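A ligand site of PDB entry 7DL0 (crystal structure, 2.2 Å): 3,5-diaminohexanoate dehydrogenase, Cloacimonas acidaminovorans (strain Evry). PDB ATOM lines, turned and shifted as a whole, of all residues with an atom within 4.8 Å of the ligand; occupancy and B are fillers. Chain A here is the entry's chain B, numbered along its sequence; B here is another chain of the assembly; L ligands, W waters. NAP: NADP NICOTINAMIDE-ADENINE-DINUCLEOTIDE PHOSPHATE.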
ATOM      1  N   ASP A  49      24.898   4.799  -5.768  1.00  0.00           N
ATOM      2  CA  ASP A  49      24.861   6.213  -5.438  1.00  0.00           C
ATOM      3  C   ASP A  49      24.927   6.428  -3.933  1.00  0.00           C
ATOM      4  O   ASP A  49      24.164   5.828  -3.163  1.00  0.00           O
ATOM      5  CB  ASP A  49      23.579   6.848  -5.995  1.00  0.00           C
ATOM      6  CG  ASP A  49      23.369   8.267  -5.479  1.00  0.00           C
ATOM      7  OD1 ASP A  49      24.052   9.215  -5.959  1.00  0.00           O
ATOM      8  OD2 ASP A  49      22.539   8.430  -4.561  1.00  0.00           O
ATOM      9  N   SER A  50      25.825   7.317  -3.515  1.00  0.00           N
ATOM     10  CA  SER A  50      26.057   7.542  -2.100  1.00  0.00           C
ATOM     11  C   SER A  50      24.780   7.892  -1.356  1.00  0.00           C
ATOM     12  O   SER A  50      24.531   7.394  -0.252  1.00  0.00           O
ATOM     13  CB  SER A  50      27.092   8.650  -1.892  1.00  0.00           C
ATOM     14  OG  SER A  50      27.179   9.005  -0.521  1.00  0.00           O
ATOM     15  N   ALA A  51      23.944   8.768  -1.924  1.00  0.00           N
ATOM     16  CA  ALA A  51      22.708   9.082  -1.241  1.00  0.00           C
ATOM     17  C   ALA A  51      21.804   7.863  -1.168  1.00  0.00           C
ATOM     18  O   ALA A  51      21.083   7.673  -0.171  1.00  0.00           O
ATOM     19  CB  ALA A  51      21.992  10.248  -1.932  1.00  0.00           C
ATOM     20  N   ASP A 177      32.397   8.170 -10.992  1.00  0.00           N
ATOM     21  CA  ASP A 177      31.066   8.292 -10.424  1.00  0.00           C
ATOM     22  C   ASP A 177      30.704   9.747 -10.142  1.00  0.00           C
ATOM     23  O   ASP A 177      29.526  10.095 -10.094  1.00  0.00           O
ATOM     24  CB  ASP A 177      30.988   7.444  -9.149  1.00  0.00           C
ATOM     25  CG  ASP A 177      29.751   7.720  -8.335  1.00  0.00           C
ATOM     26  OD1 ASP A 177      28.645   7.607  -8.895  1.00  0.00           O
ATOM     27  OD2 ASP A 177      29.888   8.033  -7.127  1.00  0.00           O
ATOM     28  N   VAL A 178      31.698  10.624  -9.954  1.00  0.00           N
ATOM     29  CA  VAL A 178      31.384  12.005  -9.579  1.00  0.00           C
ATOM     30  C   VAL A 178      32.101  12.959 -10.535  1.00  0.00           C
ATOM     31  O   VAL A 178      32.288  14.135 -10.223  1.00  0.00           O
ATOM     32  CB  VAL A 178      31.741  12.283  -8.103  1.00  0.00           C
ATOM     33  CG1 VAL A 178      30.831  11.490  -7.163  1.00  0.00           C
ATOM     34  CG2 VAL A 178      33.191  11.933  -7.832  1.00  0.00           C
ATOM     35  N   GLY A 199      29.673  19.631   2.658  1.00  0.00           N
ATOM     36  CA  GLY A 199      30.084  18.240   2.501  1.00  0.00           C
ATOM     37  C   GLY A 199      31.500  18.160   1.976  1.00  0.00           C
ATOM     38  O   GLY A 199      31.828  17.296   1.159  1.00  0.00           O
ATOM     39  N   ASN A 201      34.421  17.166   2.831  1.00  0.00           N
ATOM     40  CA  ASN A 201      35.369  16.073   2.944  1.00  0.00           C
ATOM     41  C   ASN A 201      35.014  14.897   2.043  1.00  0.00           C
ATOM     42  O   ASN A 201      35.841  13.983   1.891  1.00  0.00           O
ATOM     43  CB  ASN A 201      35.456  15.612   4.401  1.00  0.00           C
ATOM     44  CG  ASN A 201      36.558  14.601   4.651  1.00  0.00           C
ATOM     45  OD1 ASN A 201      37.761  14.879   4.435  1.00  0.00           O
ATOM     46  ND2 ASN A 201      36.169  13.431   5.151  1.00  0.00           N
ATOM     47  N   GLY A 202      33.839  14.910   1.404  1.00  0.00           N
ATOM     48  CA  GLY A 202      33.359  13.773   0.668  1.00  0.00           C
ATOM     49  C   GLY A 202      34.118  13.550  -0.625  1.00  0.00           C
ATOM     50  O   GLY A 202      35.041  14.268  -0.986  1.00  0.00           O
ATOM     51  N   LYS A 203      33.680  12.519  -1.368  1.00  0.00           N
ATOM     52  CA  LYS A 203      34.382  12.148  -2.592  1.00  0.00           C
ATOM     53  C   LYS A 203      34.301  13.267  -3.635  1.00  0.00           C
ATOM     54  O   LYS A 203      35.334  13.723  -4.139  1.00  0.00           O
ATOM     55  CB  LYS A 203      33.806  10.828  -3.142  1.00  0.00           C
ATOM     56  CG  LYS A 203      34.422  10.424  -4.473  1.00  0.00           C
ATOM     57  CD  LYS A 203      34.089   8.976  -4.933  1.00  0.00           C
ATOM     58  CE  LYS A 203      32.588   8.658  -4.961  1.00  0.00           C
ATOM     59  NZ  LYS A 203      32.256   7.286  -5.492  1.00  0.00           N
ATOM     60  N   SER A 204      33.086  13.735  -3.969  1.00  0.00           N
ATOM     61  CA  SER A 204      33.014  14.862  -4.899  1.00  0.00           C
ATOM     62  C   SER A 204      33.422  16.175  -4.238  1.00  0.00           C
ATOM     63  O   SER A 204      33.933  17.072  -4.909  1.00  0.00           O
ATOM     64  CB  SER A 204      31.609  14.977  -5.507  1.00  0.00           C
ATOM     65  OG  SER A 204      30.643  15.125  -4.496  1.00  0.00           O
ATOM     66  N   GLY A 205      33.205  16.298  -2.921  1.00  0.00           N
ATOM     67  CA  GLY A 205      33.592  17.518  -2.224  1.00  0.00           C
ATOM     68  C   GLY A 205      35.055  17.904  -2.392  1.00  0.00           C
ATOM     69  O   GLY A 205      35.369  19.060  -2.694  1.00  0.00           O
ATOM     70  N   VAL A 226      31.935  20.977   7.195  1.00  0.00           N
ATOM     71  CA  VAL A 226      32.003  19.577   7.612  1.00  0.00           C
ATOM     72  C   VAL A 226      31.521  19.512   9.061  1.00  0.00           C
ATOM     73  O   VAL A 226      31.468  20.516   9.753  1.00  0.00           O
ATOM     74  CB  VAL A 226      33.436  18.983   7.528  1.00  0.00           C
ATOM     75  CG1 VAL A 226      33.938  18.951   6.106  1.00  0.00           C
ATOM     76  CG2 VAL A 226      34.386  19.746   8.461  1.00  0.00           C
ATOM     77  N   ARG A 227      31.182  18.309   9.509  1.00  0.00           N
ATOM     78  CA  ARG A 227      30.769  18.138  10.894  1.00  0.00           C
ATOM     79  C   ARG A 227      31.766  17.355  11.733  1.00  0.00           C
ATOM     80  O   ARG A 227      31.477  17.051  12.881  1.00  0.00           O
ATOM     81  CB  ARG A 227      29.422  17.441  10.961  1.00  0.00           C
ATOM     82  CG  ARG A 227      29.405  16.081  10.291  1.00  0.00           C
ATOM     83  CD  ARG A 227      27.979  15.555  10.251  1.00  0.00           C
ATOM     84  NE  ARG A 227      27.852  14.437   9.324  1.00  0.00           N
ATOM     85  CZ  ARG A 227      26.738  13.740   9.141  1.00  0.00           C
ATOM     86  NH1 ARG A 227      25.646  14.008   9.829  1.00  0.00           N
ATOM     87  NH2 ARG A 227      26.720  12.771   8.227  1.00  0.00           N
ATOM     88  N   TYR A 231      38.197  16.256   9.789  1.00  0.00           N
ATOM     89  CA  TYR A 231      38.277  16.421   8.352  1.00  0.00           C
ATOM     90  C   TYR A 231      38.991  17.690   7.953  1.00  0.00           C
ATOM     91  O   TYR A 231      39.373  17.822   6.782  1.00  0.00           O
ATOM     92  CB  TYR A 231      36.890  16.452   7.715  1.00  0.00           C
ATOM     93  CG  TYR A 231      36.062  15.230   7.930  1.00  0.00           C
ATOM     94  CD1 TYR A 231      36.640  14.020   8.320  1.00  0.00           C
ATOM     95  CD2 TYR A 231      34.703  15.285   7.727  1.00  0.00           C
ATOM     96  CE1 TYR A 231      35.853  12.882   8.495  1.00  0.00           C
ATOM     97  CE2 TYR A 231      33.911  14.161   7.881  1.00  0.00           C
ATOM     98  CZ  TYR A 231      34.481  12.966   8.273  1.00  0.00           C
ATOM     99  OH  TYR A 231      33.652  11.868   8.435  1.00  0.00           O
ATOM    100  N   ALA A 246      29.951  22.427  11.243  1.00  0.00           N
ATOM    101  CA  ALA A 246      28.517  22.507  11.472  1.00  0.00           C
ATOM    102  C   ALA A 246      27.865  21.282  10.851  1.00  0.00           C
ATOM    103  O   ALA A 246      28.390  20.723   9.889  1.00  0.00           O
ATOM    104  CB  ALA A 246      27.905  23.783  10.864  1.00  0.00           C
ATOM    105  N   GLN A 247      26.729  20.911  11.409  1.00  0.00           N
ATOM    106  CA  GLN A 247      25.844  19.954  10.751  1.00  0.00           C
ATOM    107  C   GLN A 247      25.257  20.606   9.508  1.00  0.00           C
ATOM    108  O   GLN A 247      24.768  21.738   9.568  1.00  0.00           O
ATOM    109  CB  GLN A 247      24.719  19.551  11.706  1.00  0.00           C
ATOM    110  CG  GLN A 247      25.205  18.861  12.963  1.00  0.00           C
ATOM    111  CD  GLN A 247      25.600  17.422  12.682  1.00  0.00           C
ATOM    112  OE1 GLN A 247      25.058  16.782  11.788  1.00  0.00           O
ATOM    113  NE2 GLN A 247      26.572  16.932  13.420  1.00  0.00           N
ATOM    114  N   ALA A 248      25.314  19.905   8.377  1.00  0.00           N
ATOM    115  CA  ALA A 248      24.761  20.407   7.121  1.00  0.00           C
ATOM    116  C   ALA A 248      23.267  20.674   7.198  1.00  0.00           C
ATOM    117  O   ALA A 248      22.707  21.275   6.270  1.00  0.00           O
ATOM    118  CB  ALA A 248      25.031  19.427   5.999  1.00  0.00           C
ATOM    119  N   THR A 249      22.601  20.206   8.239  1.00  0.00           N
ATOM    120  CA  THR A 249      21.199  20.515   8.478  1.00  0.00           C
ATOM    121  C   THR A 249      21.021  21.760   9.327  1.00  0.00           C
ATOM    122  O   THR A 249      19.886  22.123   9.649  1.00  0.00           O
ATOM    123  CB  THR A 249      20.501  19.336   9.162  1.00  0.00           C
ATOM    124  OG1 THR A 249      21.262  18.957  10.316  1.00  0.00           O
ATOM    125  CG2 THR A 249      20.380  18.138   8.226  1.00  0.00           C
ATOM    126  N   VAL A 273      27.123  18.849  -1.735  1.00  0.00           N
ATOM    127  CA  VAL A 273      27.543  17.498  -2.095  1.00  0.00           C
ATOM    128  C   VAL A 273      27.396  16.567  -0.885  1.00  0.00           C
ATOM    129  O   VAL A 273      28.275  15.743  -0.621  1.00  0.00           O
ATOM    130  CB  VAL A 273      28.986  17.504  -2.626  1.00  0.00           C
ATOM    131  CG1 VAL A 273      29.043  18.116  -4.014  1.00  0.00           C
ATOM    132  CG2 VAL A 273      29.921  18.298  -1.689  1.00  0.00           C
ATOM    133  N   VAL A 274      26.359  16.756  -0.089  1.00  0.00           N
ATOM    134  CA  VAL A 274      26.141  15.826   1.015  1.00  0.00           C
ATOM    135  C   VAL A 274      25.307  14.668   0.483  1.00  0.00           C
ATOM    136  O   VAL A 274      24.923  14.650  -0.684  1.00  0.00           O
ATOM    137  CB  VAL A 274      25.487  16.506   2.233  1.00  0.00           C
ATOM    138  CG1 VAL A 274      26.487  17.428   2.900  1.00  0.00           C
ATOM    139  CG2 VAL A 274      24.286  17.282   1.836  1.00  0.00           C
ATOM    140  N   ASN A 275      25.037  13.683   1.326  1.00  0.00           N
ATOM    141  CA  ASN A 275      24.226  12.548   0.898  1.00  0.00           C
ATOM    142  C   ASN A 275      23.049  12.286   1.824  1.00  0.00           C
ATOM    143  O   ASN A 275      22.486  11.194   1.815  1.00  0.00           O
ATOM    144  CB  ASN A 275      25.093  11.286   0.728  1.00  0.00           C
ATOM    145  CG  ASN A 275      25.668  10.774   2.037  1.00  0.00           C
ATOM    146  OD1 ASN A 275      25.682  11.466   3.067  1.00  0.00           O
ATOM    147  ND2 ASN A 275      26.141   9.525   2.015  1.00  0.00           N
ATOM    148  N   THR A 276      22.636  13.313   2.575  1.00  0.00           N
ATOM    149  CA  THR A 276      21.538  13.216   3.527  1.00  0.00           C
ATOM    150  C   THR A 276      20.528  14.306   3.227  1.00  0.00           C
ATOM    151  O   THR A 276      20.791  15.270   2.503  1.00  0.00           O
ATOM    152  CB  THR A 276      22.028  13.359   4.957  1.00  0.00           C
ATOM    153  OG1 THR A 276      22.801  14.577   5.039  1.00  0.00           O
ATOM    154  CG2 THR A 276      22.873  12.166   5.370  1.00  0.00           C
ATOM    155  N   PHE A 296      24.146  19.209  -6.064  1.00  0.00           N
ATOM    156  CA  PHE A 296      24.623  17.992  -6.708  1.00  0.00           C
ATOM    157  C   PHE A 296      24.057  16.749  -6.032  1.00  0.00           C
ATOM    158  O   PHE A 296      23.905  15.716  -6.681  1.00  0.00           O
ATOM    159  CB  PHE A 296      26.161  18.002  -6.711  1.00  0.00           C
ATOM    160  CG  PHE A 296      26.792  16.928  -7.564  1.00  0.00           C
ATOM    161  CD1 PHE A 296      26.780  17.009  -8.960  1.00  0.00           C
ATOM    162  CD2 PHE A 296      27.439  15.832  -6.963  1.00  0.00           C
ATOM    163  CE1 PHE A 296      27.374  15.998  -9.746  1.00  0.00           C
ATOM    164  CE2 PHE A 296      28.041  14.822  -7.726  1.00  0.00           C
ATOM    165  CZ  PHE A 296      28.010  14.901  -9.133  1.00  0.00           C
ATOM    166  N   SER A 297      23.640  16.860  -4.777  1.00  0.00           N
ATOM    167  CA  SER A 297      23.203  15.717  -3.987  1.00  0.00           C
ATOM    168  C   SER A 297      21.898  15.127  -4.483  1.00  0.00           C
ATOM    169  O   SER A 297      20.912  15.863  -4.680  1.00  0.00           O
ATOM    170  CB  SER A 297      23.008  16.143  -2.542  1.00  0.00           C
ATOM    171  OG  SER A 297      22.316  15.137  -1.812  1.00  0.00           O
ATOM    172  N   MET A 298      21.848  13.773  -4.579  1.00  0.00           N
ATOM    173  CA  MET A 298      20.611  13.054  -4.888  1.00  0.00           C
ATOM    174  C   MET A 298      19.691  12.906  -3.692  1.00  0.00           C
ATOM    175  O   MET A 298      18.609  12.333  -3.858  1.00  0.00           O
ATOM    176  CB  MET A 298      20.885  11.668  -5.460  1.00  0.00           C
ATOM    177  CG  MET A 298      21.692  11.717  -6.723  1.00  0.00           C
ATOM    178  SD  MET A 298      20.640  12.348  -8.057  1.00  0.00           S
ATOM    179  CE  MET A 298      21.129  14.047  -8.192  1.00  0.00           C
ATOM    180  N   ALA A 299      20.077  13.377  -2.514  1.00  0.00           N
ATOM    181  CA  ALA A 299      19.159  13.521  -1.395  1.00  0.00           C
ATOM    182  C   ALA A 299      18.387  14.843  -1.417  1.00  0.00           C
ATOM    183  O   ALA A 299      17.531  15.053  -0.552  1.00  0.00           O
ATOM    184  CB  ALA A 299      19.918  13.406  -0.053  1.00  0.00           C
ATOM    185  N   GLY A 321      21.838  19.500 -10.093  1.00  0.00           N
ATOM    186  CA  GLY A 321      23.121  19.033 -10.539  1.00  0.00           C
ATOM    187  C   GLY A 321      22.999  17.999 -11.637  1.00  0.00           C
ATOM    188  O   GLY A 321      22.380  16.949 -11.447  1.00  0.00           O
ATOM    189  N   ASN A 322      23.560  18.281 -12.785  1.00  0.00           N
ATOM    190  CA  ASN A 322      23.596  17.331 -13.878  1.00  0.00           C
ATOM    191  C   ASN A 322      24.871  16.503 -13.766  1.00  0.00           C
ATOM    192  O   ASN A 322      25.978  17.058 -13.850  1.00  0.00           O
ATOM    193  CB  ASN A 322      23.532  18.041 -15.219  1.00  0.00           C
ATOM    194  CG  ASN A 322      23.269  17.089 -16.380  1.00  0.00           C
ATOM    195  OD1 ASN A 322      23.326  15.862 -16.212  1.00  0.00           O
ATOM    196  ND2 ASN A 322      22.981  17.638 -17.548  1.00  0.00           N
ATOM    197  N   GLY A 323      24.728  15.191 -13.604  1.00  0.00           N
ATOM    198  CA  GLY A 323      25.915  14.373 -13.511  1.00  0.00           C
ATOM    199  C   GLY A 323      26.689  14.224 -14.815  1.00  0.00           C
ATOM    200  O   GLY A 323      27.805  13.704 -14.778  1.00  0.00           O
ATOM    201  N   TYR A 350      40.077   4.888  -2.215  1.00  0.00           N
ATOM    202  CA  TYR A 350      39.246   4.122  -3.122  1.00  0.00           C
ATOM    203  C   TYR A 350      39.985   3.092  -3.956  1.00  0.00           C
ATOM    204  O   TYR A 350      39.338   2.262  -4.601  1.00  0.00           O
ATOM    205  CB  TYR A 350      38.465   5.074  -4.046  1.00  0.00           C
ATOM    206  CG  TYR A 350      37.783   6.195  -3.293  1.00  0.00           C
ATOM    207  CD1 TYR A 350      36.807   5.938  -2.335  1.00  0.00           C
ATOM    208  CD2 TYR A 350      38.137   7.515  -3.509  1.00  0.00           C
ATOM    209  CE1 TYR A 350      36.194   6.958  -1.638  1.00  0.00           C
ATOM    210  CE2 TYR A 350      37.536   8.542  -2.816  1.00  0.00           C
ATOM    211  CZ  TYR A 350      36.559   8.260  -1.878  1.00  0.00           C
ATOM    212  OH  TYR A 350      35.977   9.283  -1.182  1.00  0.00           O
ATOM    213  N   LEU B 307      18.885  12.782 -13.112  1.00  0.00           N
ATOM    214  CA  LEU B 307      19.306  11.527 -13.684  1.00  0.00           C
ATOM    215  C   LEU B 307      18.637  11.298 -15.036  1.00  0.00           C
ATOM    216  O   LEU B 307      19.158  10.528 -15.855  1.00  0.00           O
ATOM    217  CB  LEU B 307      19.001  10.389 -12.697  1.00  0.00           C
ATOM    218  CG  LEU B 307      19.556  10.591 -11.281  1.00  0.00           C
ATOM    219  CD1 LEU B 307      19.188   9.463 -10.360  1.00  0.00           C
ATOM    220  CD2 LEU B 307      21.051  10.708 -11.363  1.00  0.00           C
HETATM  221  PA  NAP L   1      30.256  10.891  -0.234  1.00  0.00           P
HETATM  222  O1A NAP L   1      29.522   9.992   0.688  1.00  0.00           O
HETATM  223  O2A NAP L   1      31.629  10.530  -0.665  1.00  0.00           O
HETATM  224  O5B NAP L   1      30.264  12.374   0.359  1.00  0.00           O
HETATM  225  C5B NAP L   1      29.186  12.813   1.211  1.00  0.00           C
HETATM  226  C4B NAP L   1      29.747  13.784   2.216  1.00  0.00           C
HETATM  227  O4B NAP L   1      28.672  14.493   2.863  1.00  0.00           O
HETATM  228  C3B NAP L   1      30.588  13.157   3.336  1.00  0.00           C
HETATM  229  O3B NAP L   1      31.840  13.823   3.431  1.00  0.00           O
HETATM  230  C2B NAP L   1      29.735  13.340   4.584  1.00  0.00           C
HETATM  231  O2B NAP L   1      30.559  13.610   5.719  1.00  0.00           O
HETATM  232  C1B NAP L   1      28.958  14.597   4.224  1.00  0.00           C
HETATM  233  N9A NAP L   1      27.707  14.749   4.951  1.00  0.00           N
HETATM  234  C8A NAP L   1      26.570  14.005   4.798  1.00  0.00           C
HETATM  235  N7A NAP L   1      25.602  14.390   5.589  1.00  0.00           N
HETATM  236  C5A NAP L   1      26.129  15.442   6.307  1.00  0.00           C
HETATM  237  C6A NAP L   1      25.601  16.275   7.299  1.00  0.00           C
HETATM  238  N6A NAP L   1      24.360  16.164   7.765  1.00  0.00           N
HETATM  239  N1A NAP L   1      26.405  17.219   7.824  1.00  0.00           N
HETATM  240  C2A NAP L   1      27.650  17.341   7.339  1.00  0.00           C
HETATM  241  N3A NAP L   1      28.254  16.622   6.406  1.00  0.00           N
HETATM  242  C4A NAP L   1      27.434  15.671   5.920  1.00  0.00           C
HETATM  243  O3  NAP L   1      29.357  11.111  -1.524  1.00  0.00           O
HETATM  244  PN  NAP L   1      29.758  11.542  -3.000  1.00  0.00           P
HETATM  245  O1N NAP L   1      30.097  10.327  -3.775  1.00  0.00           O
HETATM  246  O2N NAP L   1      30.745  12.644  -2.918  1.00  0.00           O
HETATM  247  O5D NAP L   1      28.369  12.125  -3.511  1.00  0.00           O
HETATM  248  C5D NAP L   1      27.924  13.362  -2.939  1.00  0.00           C
HETATM  249  C4D NAP L   1      26.473  13.595  -3.301  1.00  0.00           C
HETATM  250  O4D NAP L   1      26.372  13.728  -4.729  1.00  0.00           O
HETATM  251  C3D NAP L   1      25.510  12.476  -2.901  1.00  0.00           C
HETATM  252  O3D NAP L   1      24.310  13.009  -2.355  1.00  0.00           O
HETATM  253  C2D NAP L   1      25.275  11.748  -4.214  1.00  0.00           C
HETATM  254  O2D NAP L   1      23.984  11.167  -4.267  1.00  0.00           O
HETATM  255  C1D NAP L   1      25.357  12.878  -5.229  1.00  0.00           C
HETATM  256  N1N NAP L   1      25.756  12.402  -6.573  1.00  0.00           N
HETATM  257  C2N NAP L   1      25.046  12.822  -7.659  1.00  0.00           C
HETATM  258  C3N NAP L   1      25.430  12.465  -8.936  1.00  0.00           C
HETATM  259  C7N NAP L   1      24.695  13.090 -10.091  1.00  0.00           C
HETATM  260  O7N NAP L   1      24.490  12.433 -11.106  1.00  0.00           O
HETATM  261  N7N NAP L   1      24.281  14.341  -9.965  1.00  0.00           N
HETATM  262  C4N NAP L   1      26.461  11.547  -9.087  1.00  0.00           C
HETATM  263  C5N NAP L   1      27.117  11.070  -7.977  1.00  0.00           C
HETATM  264  C6N NAP L   1      26.783  11.556  -6.745  1.00  0.00           C
HETATM  265  P2B NAP L   1      30.287  12.645   6.976  1.00  0.00           P
HETATM  266  O1X NAP L   1      28.957  11.961   6.822  1.00  0.00           O
HETATM  267  O2X NAP L   1      31.418  11.659   7.009  1.00  0.00           O
HETATM  268  O3X NAP L   1      30.321  13.573   8.140  1.00  0.00           O
HETATM  269  O   HOH W   1      27.992   8.882  -5.134  1.00  0.00           O
HETATM  270  O   HOH W   2      21.783  14.707   8.847  1.00  0.00           O
HETATM  271  O   HOH W   3      31.155  15.013  -1.230  1.00  0.00           O
HETATM  272  O   HOH W   4      31.035  16.381   7.131  1.00  0.00           O
HETATM  273  O   HOH W   5      23.029  16.979  10.225  1.00  0.00           O
HETATM  274  O   HOH W   6      31.464  12.748  10.705  1.00  0.00           O
HETATM  275  O   HOH W   7      31.987  16.336   4.604  1.00  0.00           O
HETATM  276  O   HOH W   8      29.758   9.555   3.227  1.00  0.00           O
HETATM  277  O   HOH W   9      33.732   9.293   0.677  1.00  0.00           O
HETATM  278  O   HOH W  10      33.476  12.137   4.809  1.00  0.00           O
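O2A of the ligand is in hydrogen-bond range of N of Lys 203 (2.9 Å). The backbone NH (N) of Ala 248 is in hydrogen-bond range of a nitrogen (N1A) of the ligand (3.0 Å). An oxygen (O2N) of the ligand is in hydrogen-bond range of the side-chain hydroxyl (OG) of Ser 204 (2.9 Å). The side-chain carboxylate (OD1) of Asp 49 lies within hydrogen-bond range of an oxygen (O2D) of the ligand (2.6 Å). The side-chain hydroxyl (OG1) of Thr 276 lies within hydrogen-bond range of a nitrogen (N7A) of the ligand, at 2.9 Å. The backbone NH of Met 298 lies close to an oxygen (O2D) of the ligand (3.4 Å). The backbone NH (N) of Ala 51 lies close to an oxygen (O2D) of the ligand, 3.4 Å away. N of Gly 202 lies within hydrogen-bond range of O3B of the ligand, 3.0 Å away. The backbone carbonyl oxygen of Val 274 is in hydrogen-bond range of an oxygen (O3D) of the ligand. The backbone NH (N) of Ser 204 is in hydrogen-bond range of an oxygen (O2N) of the ligand, 2.8 Å away. The side-chain hydroxyl of Ser 50 is in hydrogen-bond range of an oxygen (O1A) of the ligand. NH2 of Arg 227 is in salt-bridge range of O1X of the ligand (2.8 Å). OH of Tyr 231 sits at hydrogen-bond distance from O2X of the ligand. The side-chain hydroxyl (OG) of Ser 297 lies within hydrogen-bond range of an oxygen (O3D) of the ligand, 3.0 Å away.
The side-chain hydroxyl (OG) of Ser 50 lies within hydrogen-bond range of the side-chain amide nitrogen (ND2) of Asn 275, at 2.8 Å. O of Val 274 is in hydrogen-bond range of OG of Ser 297, at 2.9 Å. OD2 of Asp 177 lies within salt-bridge range of NZ of Lys 203, at 3.0 Å. The side-chain hydroxyl (OG) of Ser 297 lies within hydrogen-bond range of the backbone NH (N) of Ala 299, 2.9 Å away. The side-chain carboxylate of Asp 49 is in hydrogen-bond range of the backbone NH of Ala 51 (3.0 Å). The guanidinium group (NH1) of Arg 227 sits at hydrogen-bond distance from the side-chain amide oxygen (OE1) of Gln 247.
O of Asp 177 touches C5N of the ligand, at 3.4 Å. Val 178 touches the ligand. Asn 201 touches the ligand. C of Gln 247 touches N1A of the ligand (3.95 Å). O of Val 273 touches C5D of the ligand, at 3.3 Å. Asn 275 touches the ligand (OD1 to C8A, 3.2 Å). Phe 296 touches the ligand (CD2 to O4D, 3.2 Å). O of Gly 321 touches N7N of the ligand (3.6 Å). CA of Gly 323 touches O7N of the ligand, at 3.4 Å. CD2 of Leu 307 of chain B touches O7N of the ligand, at 3.9 Å. Hydrophobic or aromatic side chains within 4 Å of the ligand: Ala 51, Val 178, Tyr 231, Ala 248, Val 274, Phe 296, Met 298 and Leu 307 of chain B. 23 residues have an atom within 4 Å of the ligand: Asp 49, Ser 50, Ala 51, Asp 177, Val 178, Asn 201, Gly 202, Lys 203, Ser 204, Arg 227, Tyr 231, Gln 247, Ala 248, Val 273, Val 274, Asn 275, Thr 276, Phe 296, Ser 297, Met 298, Gly 321, Gly 323 and Leu 307 of chain B.
Water W10 bridges O3B of the ligand and ND2 of Asn 201. Water W7 bridges O3B of the ligand (2.8 Å) and N of Asn 201 (3.1 Å). Water W9 lies within hydrogen-bond range of an oxygen (O2A) of the ligand and the side-chain hydroxyl of Tyr 350. Water W4 bridges N3A of the ligand (2.9 Å) and N of Arg 227 (3.1 Å). Water W1 lies within hydrogen-bond range of OD2 of Asp 177 (2.9 Å), O1N of the ligand (2.9 Å) and N of Ser 50 (3.1 Å). Water W5 lies within hydrogen-bond range of the side-chain amide oxygen of Gln 247 (2.6 Å), the side-chain hydroxyl of Thr 249 (2.7 Å) and a nitrogen (N6A) of the ligand (2.9 Å).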
